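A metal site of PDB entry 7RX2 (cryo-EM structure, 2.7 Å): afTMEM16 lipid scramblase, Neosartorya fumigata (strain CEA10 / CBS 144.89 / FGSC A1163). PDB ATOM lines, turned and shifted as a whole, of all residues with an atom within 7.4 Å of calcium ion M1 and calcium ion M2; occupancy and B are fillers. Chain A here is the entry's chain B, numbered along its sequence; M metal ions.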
ATOM      1  N   TYR A 180     -27.501 -23.439 -16.448  1.00  0.00           N
ATOM      2  CA  TYR A 180     -27.706 -23.926 -15.094  1.00  0.00           C
ATOM      3  C   TYR A 180     -26.976 -23.061 -14.074  1.00  0.00           C
ATOM      4  O   TYR A 180     -27.537 -22.714 -13.041  1.00  0.00           O
ATOM      5  CB  TYR A 180     -27.263 -25.378 -14.974  1.00  0.00           C
ATOM      6  CG  TYR A 180     -27.048 -25.821 -13.552  1.00  0.00           C
ATOM      7  CD1 TYR A 180     -28.110 -25.897 -12.670  1.00  0.00           C
ATOM      8  CD2 TYR A 180     -25.793 -26.126 -13.086  1.00  0.00           C
ATOM      9  CE1 TYR A 180     -27.921 -26.281 -11.374  1.00  0.00           C
ATOM     10  CE2 TYR A 180     -25.596 -26.513 -11.786  1.00  0.00           C
ATOM     11  CZ  TYR A 180     -26.659 -26.586 -10.941  1.00  0.00           C
ATOM     12  OH  TYR A 180     -26.470 -26.970  -9.645  1.00  0.00           O
ATOM     13  N   LEU A 184     -28.630 -20.916 -11.199  1.00  0.00           N
ATOM     14  CA  LEU A 184     -28.273 -21.149  -9.804  1.00  0.00           C
ATOM     15  C   LEU A 184     -27.738 -19.891  -9.140  1.00  0.00           C
ATOM     16  O   LEU A 184     -28.018 -19.652  -7.970  1.00  0.00           O
ATOM     17  CB  LEU A 184     -27.247 -22.267  -9.718  1.00  0.00           C
ATOM     18  CG  LEU A 184     -26.762 -22.629  -8.323  1.00  0.00           C
ATOM     19  CD1 LEU A 184     -27.947 -22.953  -7.463  1.00  0.00           C
ATOM     20  CD2 LEU A 184     -25.828 -23.790  -8.388  1.00  0.00           C
ATOM     21  N   ALA A 437     -30.821 -33.231   4.737  1.00  0.00           N
ATOM     22  CA  ALA A 437     -30.786 -33.779   3.391  1.00  0.00           C
ATOM     23  C   ALA A 437     -29.908 -32.961   2.455  1.00  0.00           C
ATOM     24  O   ALA A 437     -29.419 -33.498   1.465  1.00  0.00           O
ATOM     25  CB  ALA A 437     -32.198 -33.869   2.821  1.00  0.00           C
ATOM     26  N   GLN A 438     -29.698 -31.677   2.750  1.00  0.00           N
ATOM     27  CA  GLN A 438     -28.754 -30.907   1.958  1.00  0.00           C
ATOM     28  C   GLN A 438     -27.317 -31.184   2.358  1.00  0.00           C
ATOM     29  O   GLN A 438     -26.414 -31.117   1.513  1.00  0.00           O
ATOM     30  CB  GLN A 438     -29.049 -29.407   2.080  1.00  0.00           C
ATOM     31  CG  GLN A 438     -30.518 -29.038   1.961  1.00  0.00           C
ATOM     32  CD  GLN A 438     -31.103 -29.378   0.611  1.00  0.00           C
ATOM     33  OE1 GLN A 438     -32.093 -30.090   0.523  1.00  0.00           O
ATOM     34  NE2 GLN A 438     -30.500 -28.855  -0.443  1.00  0.00           N
ATOM     35  N   ILE A 439     -27.083 -31.509   3.628  1.00  0.00           N
ATOM     36  CA  ILE A 439     -25.738 -31.861   4.080  1.00  0.00           C
ATOM     37  C   ILE A 439     -25.404 -33.288   3.692  1.00  0.00           C
ATOM     38  O   ILE A 439     -24.320 -33.569   3.169  1.00  0.00           O
ATOM     39  CB  ILE A 439     -25.616 -31.637   5.600  1.00  0.00           C
ATOM     40  CG1 ILE A 439     -25.932 -30.180   5.934  1.00  0.00           C
ATOM     41  CG2 ILE A 439     -24.236 -32.013   6.082  1.00  0.00           C
ATOM     42  CD1 ILE A 439     -25.668 -29.820   7.368  1.00  0.00           C
ATOM     43  N   VAL A 440     -26.328 -34.218   3.924  1.00  0.00           N
ATOM     44  CA  VAL A 440     -26.091 -35.599   3.520  1.00  0.00           C
ATOM     45  C   VAL A 440     -26.000 -35.706   2.008  1.00  0.00           C
ATOM     46  O   VAL A 440     -25.118 -36.392   1.472  1.00  0.00           O
ATOM     47  CB  VAL A 440     -27.200 -36.520   4.065  1.00  0.00           C
ATOM     48  CG1 VAL A 440     -27.253 -37.799   3.252  1.00  0.00           C
ATOM     49  CG2 VAL A 440     -26.958 -36.823   5.534  1.00  0.00           C
ATOM     50  N   GLY A 441     -26.892 -35.032   1.290  1.00  0.00           N
ATOM     51  CA  GLY A 441     -26.867 -35.080  -0.163  1.00  0.00           C
ATOM     52  C   GLY A 441     -25.618 -34.499  -0.775  1.00  0.00           C
ATOM     53  O   GLY A 441     -25.206 -34.954  -1.856  1.00  0.00           O
ATOM     54  N   PHE A 442     -25.003 -33.521  -0.127  1.00  0.00           N
ATOM     55  CA  PHE A 442     -23.716 -33.007  -0.596  1.00  0.00           C
ATOM     56  C   PHE A 442     -22.639 -34.085  -0.575  1.00  0.00           C
ATOM     57  O   PHE A 442     -21.743 -34.073  -1.416  1.00  0.00           O
ATOM     58  CB  PHE A 442     -23.302 -31.816   0.253  1.00  0.00           C
ATOM     59  CG  PHE A 442     -21.854 -31.466   0.135  1.00  0.00           C
ATOM     60  CD1 PHE A 442     -21.380 -30.769  -0.955  1.00  0.00           C
ATOM     61  CD2 PHE A 442     -20.975 -31.818   1.142  1.00  0.00           C
ATOM     62  CE1 PHE A 442     -20.051 -30.448  -1.052  1.00  0.00           C
ATOM     63  CE2 PHE A 442     -19.633 -31.498   1.043  1.00  0.00           C
ATOM     64  CZ  PHE A 442     -19.173 -30.810  -0.048  1.00  0.00           C
ATOM     65  N   ALA A 443     -22.728 -35.022   0.373  1.00  0.00           N
ATOM     66  CA  ALA A 443     -21.738 -36.084   0.489  1.00  0.00           C
ATOM     67  C   ALA A 443     -21.878 -37.126  -0.601  1.00  0.00           C
ATOM     68  O   ALA A 443     -20.888 -37.513  -1.221  1.00  0.00           O
ATOM     69  CB  ALA A 443     -21.831 -36.740   1.870  1.00  0.00           C
ATOM     70  N   GLU A 445     -23.202 -36.696  -3.437  1.00  0.00           N
ATOM     71  CA  GLU A 445     -23.170 -36.077  -4.758  1.00  0.00           C
ATOM     72  C   GLU A 445     -21.757 -35.796  -5.235  1.00  0.00           C
ATOM     73  O   GLU A 445     -21.451 -36.011  -6.417  1.00  0.00           O
ATOM     74  CB  GLU A 445     -23.974 -34.773  -4.735  1.00  0.00           C
ATOM     75  CG  GLU A 445     -24.099 -34.097  -6.085  1.00  0.00           C
ATOM     76  CD  GLU A 445     -24.936 -32.840  -6.012  1.00  0.00           C
ATOM     77  OE1 GLU A 445     -25.479 -32.558  -4.923  1.00  0.00           O
ATOM     78  OE2 GLU A 445     -25.033 -32.137  -7.033  1.00  0.00           O
ATOM     79  N   THR A 446     -20.874 -35.332  -4.355  1.00  0.00           N
ATOM     80  CA  THR A 446     -19.542 -34.893  -4.777  1.00  0.00           C
ATOM     81  C   THR A 446     -18.411 -35.632  -4.088  1.00  0.00           C
ATOM     82  O   THR A 446     -17.349 -35.820  -4.687  1.00  0.00           O
ATOM     83  CB  THR A 446     -19.392 -33.393  -4.533  1.00  0.00           C
ATOM     84  OG1 THR A 446     -20.564 -32.718  -5.006  1.00  0.00           O
ATOM     85  CG2 THR A 446     -18.178 -32.859  -5.272  1.00  0.00           C
ATOM     86  N   TYR A 506     -21.659 -36.637 -17.078  1.00  0.00           N
ATOM     87  CA  TYR A 506     -22.400 -35.517 -16.452  1.00  0.00           C
ATOM     88  C   TYR A 506     -23.703 -35.229 -17.208  1.00  0.00           C
ATOM     89  O   TYR A 506     -23.728 -35.240 -18.458  1.00  0.00           O
ATOM     90  CB  TYR A 506     -21.527 -34.257 -16.430  1.00  0.00           C
ATOM     91  CG  TYR A 506     -22.186 -33.060 -15.799  1.00  0.00           C
ATOM     92  CD1 TYR A 506     -22.301 -32.953 -14.428  1.00  0.00           C
ATOM     93  CD2 TYR A 506     -22.733 -32.053 -16.578  1.00  0.00           C
ATOM     94  CE1 TYR A 506     -22.912 -31.864 -13.834  1.00  0.00           C
ATOM     95  CE2 TYR A 506     -23.355 -30.957 -16.001  1.00  0.00           C
ATOM     96  CZ  TYR A 506     -23.454 -30.864 -14.624  1.00  0.00           C
ATOM     97  OH  TYR A 506     -24.056 -29.789 -14.052  1.00  0.00           O
ATOM     98  N   ASP A 510     -29.799 -33.469 -13.812  1.00  0.00           N
ATOM     99  CA  ASP A 510     -29.758 -33.991 -12.423  1.00  0.00           C
ATOM    100  C   ASP A 510     -29.574 -32.796 -11.469  1.00  0.00           C
ATOM    101  O   ASP A 510     -30.212 -32.785 -10.403  1.00  0.00           O
ATOM    102  CB  ASP A 510     -28.645 -35.025 -12.238  1.00  0.00           C
ATOM    103  CG  ASP A 510     -28.808 -36.247 -13.121  1.00  0.00           C
ATOM    104  OD1 ASP A 510     -29.860 -36.375 -13.766  1.00  0.00           O
ATOM    105  OD2 ASP A 510     -27.867 -37.073 -13.144  1.00  0.00           O
ATOM    106  N   ASP A 511     -28.723 -31.840 -11.868  1.00  0.00           N
ATOM    107  CA  ASP A 511     -28.444 -30.628 -11.044  1.00  0.00           C
ATOM    108  C   ASP A 511     -29.671 -29.725 -11.047  1.00  0.00           C
ATOM    109  O   ASP A 511     -30.059 -29.254  -9.958  1.00  0.00           O
ATOM    110  CB  ASP A 511     -27.196 -29.899 -11.537  1.00  0.00           C
ATOM    111  CG  ASP A 511     -25.906 -30.513 -11.027  1.00  0.00           C
ATOM    112  OD1 ASP A 511     -25.929 -31.104  -9.929  1.00  0.00           O
ATOM    113  OD2 ASP A 511     -24.885 -30.413 -11.730  1.00  0.00           O
ATOM    114  N   LEU A 512     -30.262 -29.467 -12.221  1.00  0.00           N
ATOM    115  CA  LEU A 512     -31.449 -28.633 -12.305  1.00  0.00           C
ATOM    116  C   LEU A 512     -32.598 -29.230 -11.527  1.00  0.00           C
ATOM    117  O   LEU A 512     -33.368 -28.498 -10.912  1.00  0.00           O
ATOM    118  CB  LEU A 512     -31.856 -28.449 -13.762  1.00  0.00           C
ATOM    119  CG  LEU A 512     -31.114 -27.367 -14.538  1.00  0.00           C
ATOM    120  CD1 LEU A 512     -31.383 -27.509 -16.010  1.00  0.00           C
ATOM    121  CD2 LEU A 512     -31.520 -26.013 -14.047  1.00  0.00           C
ATOM    122  N   GLU A 514     -32.400 -31.065  -8.807  1.00  0.00           N
ATOM    123  CA  GLU A 514     -32.156 -30.912  -7.386  1.00  0.00           C
ATOM    124  C   GLU A 514     -32.415 -29.487  -6.922  1.00  0.00           C
ATOM    125  O   GLU A 514     -32.846 -29.288  -5.782  1.00  0.00           O
ATOM    126  CB  GLU A 514     -30.734 -31.335  -7.078  1.00  0.00           C
ATOM    127  CG  GLU A 514     -30.311 -31.097  -5.671  1.00  0.00           C
ATOM    128  CD  GLU A 514     -28.822 -31.253  -5.498  1.00  0.00           C
ATOM    129  OE1 GLU A 514     -28.367 -31.466  -4.355  1.00  0.00           O
ATOM    130  OE2 GLU A 514     -28.108 -31.160  -6.516  1.00  0.00           O
ATOM    131  N   MET A 515     -32.153 -28.496  -7.771  1.00  0.00           N
ATOM    132  CA  MET A 515     -32.392 -27.110  -7.380  1.00  0.00           C
ATOM    133  C   MET A 515     -33.877 -26.773  -7.407  1.00  0.00           C
ATOM    134  O   MET A 515     -34.348 -25.995  -6.583  1.00  0.00           O
ATOM    135  CB  MET A 515     -31.623 -26.163  -8.291  1.00  0.00           C
ATOM    136  CG  MET A 515     -30.192 -25.931  -7.878  1.00  0.00           C
ATOM    137  SD  MET A 515     -29.991 -25.552  -6.130  1.00  0.00           S
ATOM    138  CE  MET A 515     -29.355 -27.095  -5.515  1.00  0.00           C
ATOM    139  N   GLN A 518     -35.537 -28.415  -4.490  1.00  0.00           N
ATOM    140  CA  GLN A 518     -35.231 -27.610  -3.318  1.00  0.00           C
ATOM    141  C   GLN A 518     -36.095 -26.364  -3.266  1.00  0.00           C
ATOM    142  O   GLN A 518     -36.507 -25.943  -2.183  1.00  0.00           O
ATOM    143  CB  GLN A 518     -33.748 -27.246  -3.307  1.00  0.00           C
ATOM    144  CG  GLN A 518     -33.347 -26.441  -2.132  1.00  0.00           C
ATOM    145  CD  GLN A 518     -32.117 -25.631  -2.374  1.00  0.00           C
ATOM    146  OE1 GLN A 518     -32.190 -24.531  -2.909  1.00  0.00           O
ATOM    147  NE2 GLN A 518     -30.976 -26.152  -1.990  1.00  0.00           N
ATOM    148  N   ASN A 539     -26.451 -23.279   1.447  1.00  0.00           N
ATOM    149  CA  ASN A 539     -26.227 -24.468   0.641  1.00  0.00           C
ATOM    150  C   ASN A 539     -25.935 -24.115  -0.806  1.00  0.00           C
ATOM    151  O   ASN A 539     -25.067 -24.722  -1.440  1.00  0.00           O
ATOM    152  CB  ASN A 539     -27.435 -25.394   0.726  1.00  0.00           C
ATOM    153  CG  ASN A 539     -27.301 -26.600  -0.160  1.00  0.00           C
ATOM    154  OD1 ASN A 539     -26.714 -27.599   0.235  1.00  0.00           O
ATOM    155  ND2 ASN A 539     -27.843 -26.516  -1.365  1.00  0.00           N
ATOM    156  N   ASN A 540     -26.657 -23.145  -1.353  1.00  0.00           N
ATOM    157  CA  ASN A 540     -26.525 -22.844  -2.764  1.00  0.00           C
ATOM    158  C   ASN A 540     -25.222 -22.144  -3.103  1.00  0.00           C
ATOM    159  O   ASN A 540     -24.777 -22.235  -4.251  1.00  0.00           O
ATOM    160  CB  ASN A 540     -27.703 -22.006  -3.243  1.00  0.00           C
ATOM    161  CG  ASN A 540     -28.964 -22.817  -3.372  1.00  0.00           C
ATOM    162  OD1 ASN A 540     -28.966 -24.021  -3.148  1.00  0.00           O
ATOM    163  ND2 ASN A 540     -30.053 -22.150  -3.727  1.00  0.00           N
ATOM    164  N   VAL A 542     -22.291 -22.995  -1.649  1.00  0.00           N
ATOM    165  CA  VAL A 542     -21.432 -24.167  -1.756  1.00  0.00           C
ATOM    166  C   VAL A 542     -21.785 -24.991  -2.979  1.00  0.00           C
ATOM    167  O   VAL A 542     -20.895 -25.522  -3.650  1.00  0.00           O
ATOM    168  CB  VAL A 542     -21.534 -25.020  -0.479  1.00  0.00           C
ATOM    169  CG1 VAL A 542     -20.655 -26.222  -0.595  1.00  0.00           C
ATOM    170  CG2 VAL A 542     -21.176 -24.202   0.732  1.00  0.00           C
ATOM    171  N   GLU A 543     -23.076 -25.115  -3.286  1.00  0.00           N
ATOM    172  CA  GLU A 543     -23.507 -25.963  -4.394  1.00  0.00           C
ATOM    173  C   GLU A 543     -22.919 -25.502  -5.716  1.00  0.00           C
ATOM    174  O   GLU A 543     -22.562 -26.313  -6.567  1.00  0.00           O
ATOM    175  CB  GLU A 543     -25.028 -25.990  -4.469  1.00  0.00           C
ATOM    176  CG  GLU A 543     -25.571 -26.957  -5.490  1.00  0.00           C
ATOM    177  CD  GLU A 543     -25.842 -28.304  -4.893  1.00  0.00           C
ATOM    178  OE1 GLU A 543     -25.873 -28.389  -3.661  1.00  0.00           O
ATOM    179  OE2 GLU A 543     -26.016 -29.274  -5.647  1.00  0.00           O
ATOM    180  N   LEU A 544     -22.821 -24.192  -5.904  1.00  0.00           N
ATOM    181  CA  LEU A 544     -22.248 -23.677  -7.133  1.00  0.00           C
ATOM    182  C   LEU A 544     -20.781 -24.011  -7.255  1.00  0.00           C
ATOM    183  O   LEU A 544     -20.278 -24.229  -8.365  1.00  0.00           O
ATOM    184  CB  LEU A 544     -22.476 -22.168  -7.199  1.00  0.00           C
ATOM    185  CG  LEU A 544     -22.302 -21.534  -8.568  1.00  0.00           C
ATOM    186  CD1 LEU A 544     -23.185 -20.338  -8.669  1.00  0.00           C
ATOM    187  CD2 LEU A 544     -20.843 -21.155  -8.769  1.00  0.00           C
ATOM    188  N   SER A 546     -19.221 -26.718  -5.646  1.00  0.00           N
ATOM    189  CA  SER A 546     -19.050 -28.163  -5.713  1.00  0.00           C
ATOM    190  C   SER A 546     -19.674 -28.773  -6.959  1.00  0.00           C
ATOM    191  O   SER A 546     -19.255 -29.857  -7.372  1.00  0.00           O
ATOM    192  CB  SER A 546     -19.650 -28.818  -4.471  1.00  0.00           C
ATOM    193  OG  SER A 546     -21.053 -28.892  -4.565  1.00  0.00           O
ATOM    194  N   ASP A 547     -20.659 -28.117  -7.571  1.00  0.00           N
ATOM    195  CA  ASP A 547     -21.159 -28.587  -8.851  1.00  0.00           C
ATOM    196  C   ASP A 547     -20.167 -28.300  -9.970  1.00  0.00           C
ATOM    197  O   ASP A 547     -20.062 -29.087 -10.913  1.00  0.00           O
ATOM    198  CB  ASP A 547     -22.503 -27.950  -9.179  1.00  0.00           C
ATOM    199  CG  ASP A 547     -23.659 -28.761  -8.659  1.00  0.00           C
ATOM    200  OD1 ASP A 547     -23.452 -29.886  -8.178  1.00  0.00           O
ATOM    201  OD2 ASP A 547     -24.803 -28.259  -8.726  1.00  0.00           O
ATOM    202  N   LYS A 550     -17.463 -30.867  -9.468  1.00  0.00           N
ATOM    203  CA  LYS A 550     -17.904 -32.175  -9.932  1.00  0.00           C
ATOM    204  C   LYS A 550     -17.791 -32.318 -11.439  1.00  0.00           C
ATOM    205  O   LYS A 550     -17.492 -33.412 -11.939  1.00  0.00           O
ATOM    206  CB  LYS A 550     -19.345 -32.419  -9.489  1.00  0.00           C
ATOM    207  CG  LYS A 550     -20.078 -33.407 -10.347  1.00  0.00           C
ATOM    208  CD  LYS A 550     -21.253 -34.002  -9.625  1.00  0.00           C
ATOM    209  CE  LYS A 550     -22.300 -32.965  -9.336  1.00  0.00           C
ATOM    210  NZ  LYS A 550     -23.069 -32.605 -10.541  1.00  0.00           N
HETATM  211 CA    CA M   1     -26.255 -30.270  -7.833  1.00  0.00          CA
HETATM  212 CA    CA M   2     -26.347 -30.726  -3.316  1.00  0.00          CA
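The side-chain carboxylate (OD2) of Asp 511 lies within salt-bridge range of the side-chain amino group (NZ) of Lys 550, 3.1 Å away. OD2 of Asp 511 lies within hydrogen-bond range of OH of Tyr 506 (2.5 Å). OD1 of Asp 547 sits close to NZ of Lys 550 (3.6 Å).
Merely in contact with calcium ion M1: Tyr 180 (3.8 Å). Six residues have an atom within 4 Å of calcium ion M1: Tyr 180, Glu 445, Asp 511, Glu 514, Glu 543 and Asp 547.
The nearest printed residue that does not touch calcium ion M2 is Phe 442 (4.4 Å).
Calcium ion M1 is bound by the side-chain carboxylate (OD1) of Asp 511 (2.3 Å), the side-chain carboxylate (OE2) of Glu 445 (2.4 Å), the side-chain carboxylate (OE2) of Glu 543 (2.4 Å), the side-chain carboxylate (OE2) of Glu 514 (2.4 Å), the side-chain carboxylate (OD2) of Asp 547 (2.6 Å) and the side-chain carboxylate (OD1) of Asp 547 (2.9 Å).
Calcium ion M2 is bound by the side-chain carboxylate (OE1) of Glu 514 (2.4 Å), the side-chain carboxylate (OE1) of Glu 543 (2.4 Å), the side-chain carboxylate (OE1) of Glu 445 (2.6 Å) and the side-chain carboxylate (OE2) of Glu 543 (2.8 Å). Calcium ion M2 has four donor atoms within binding distance.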
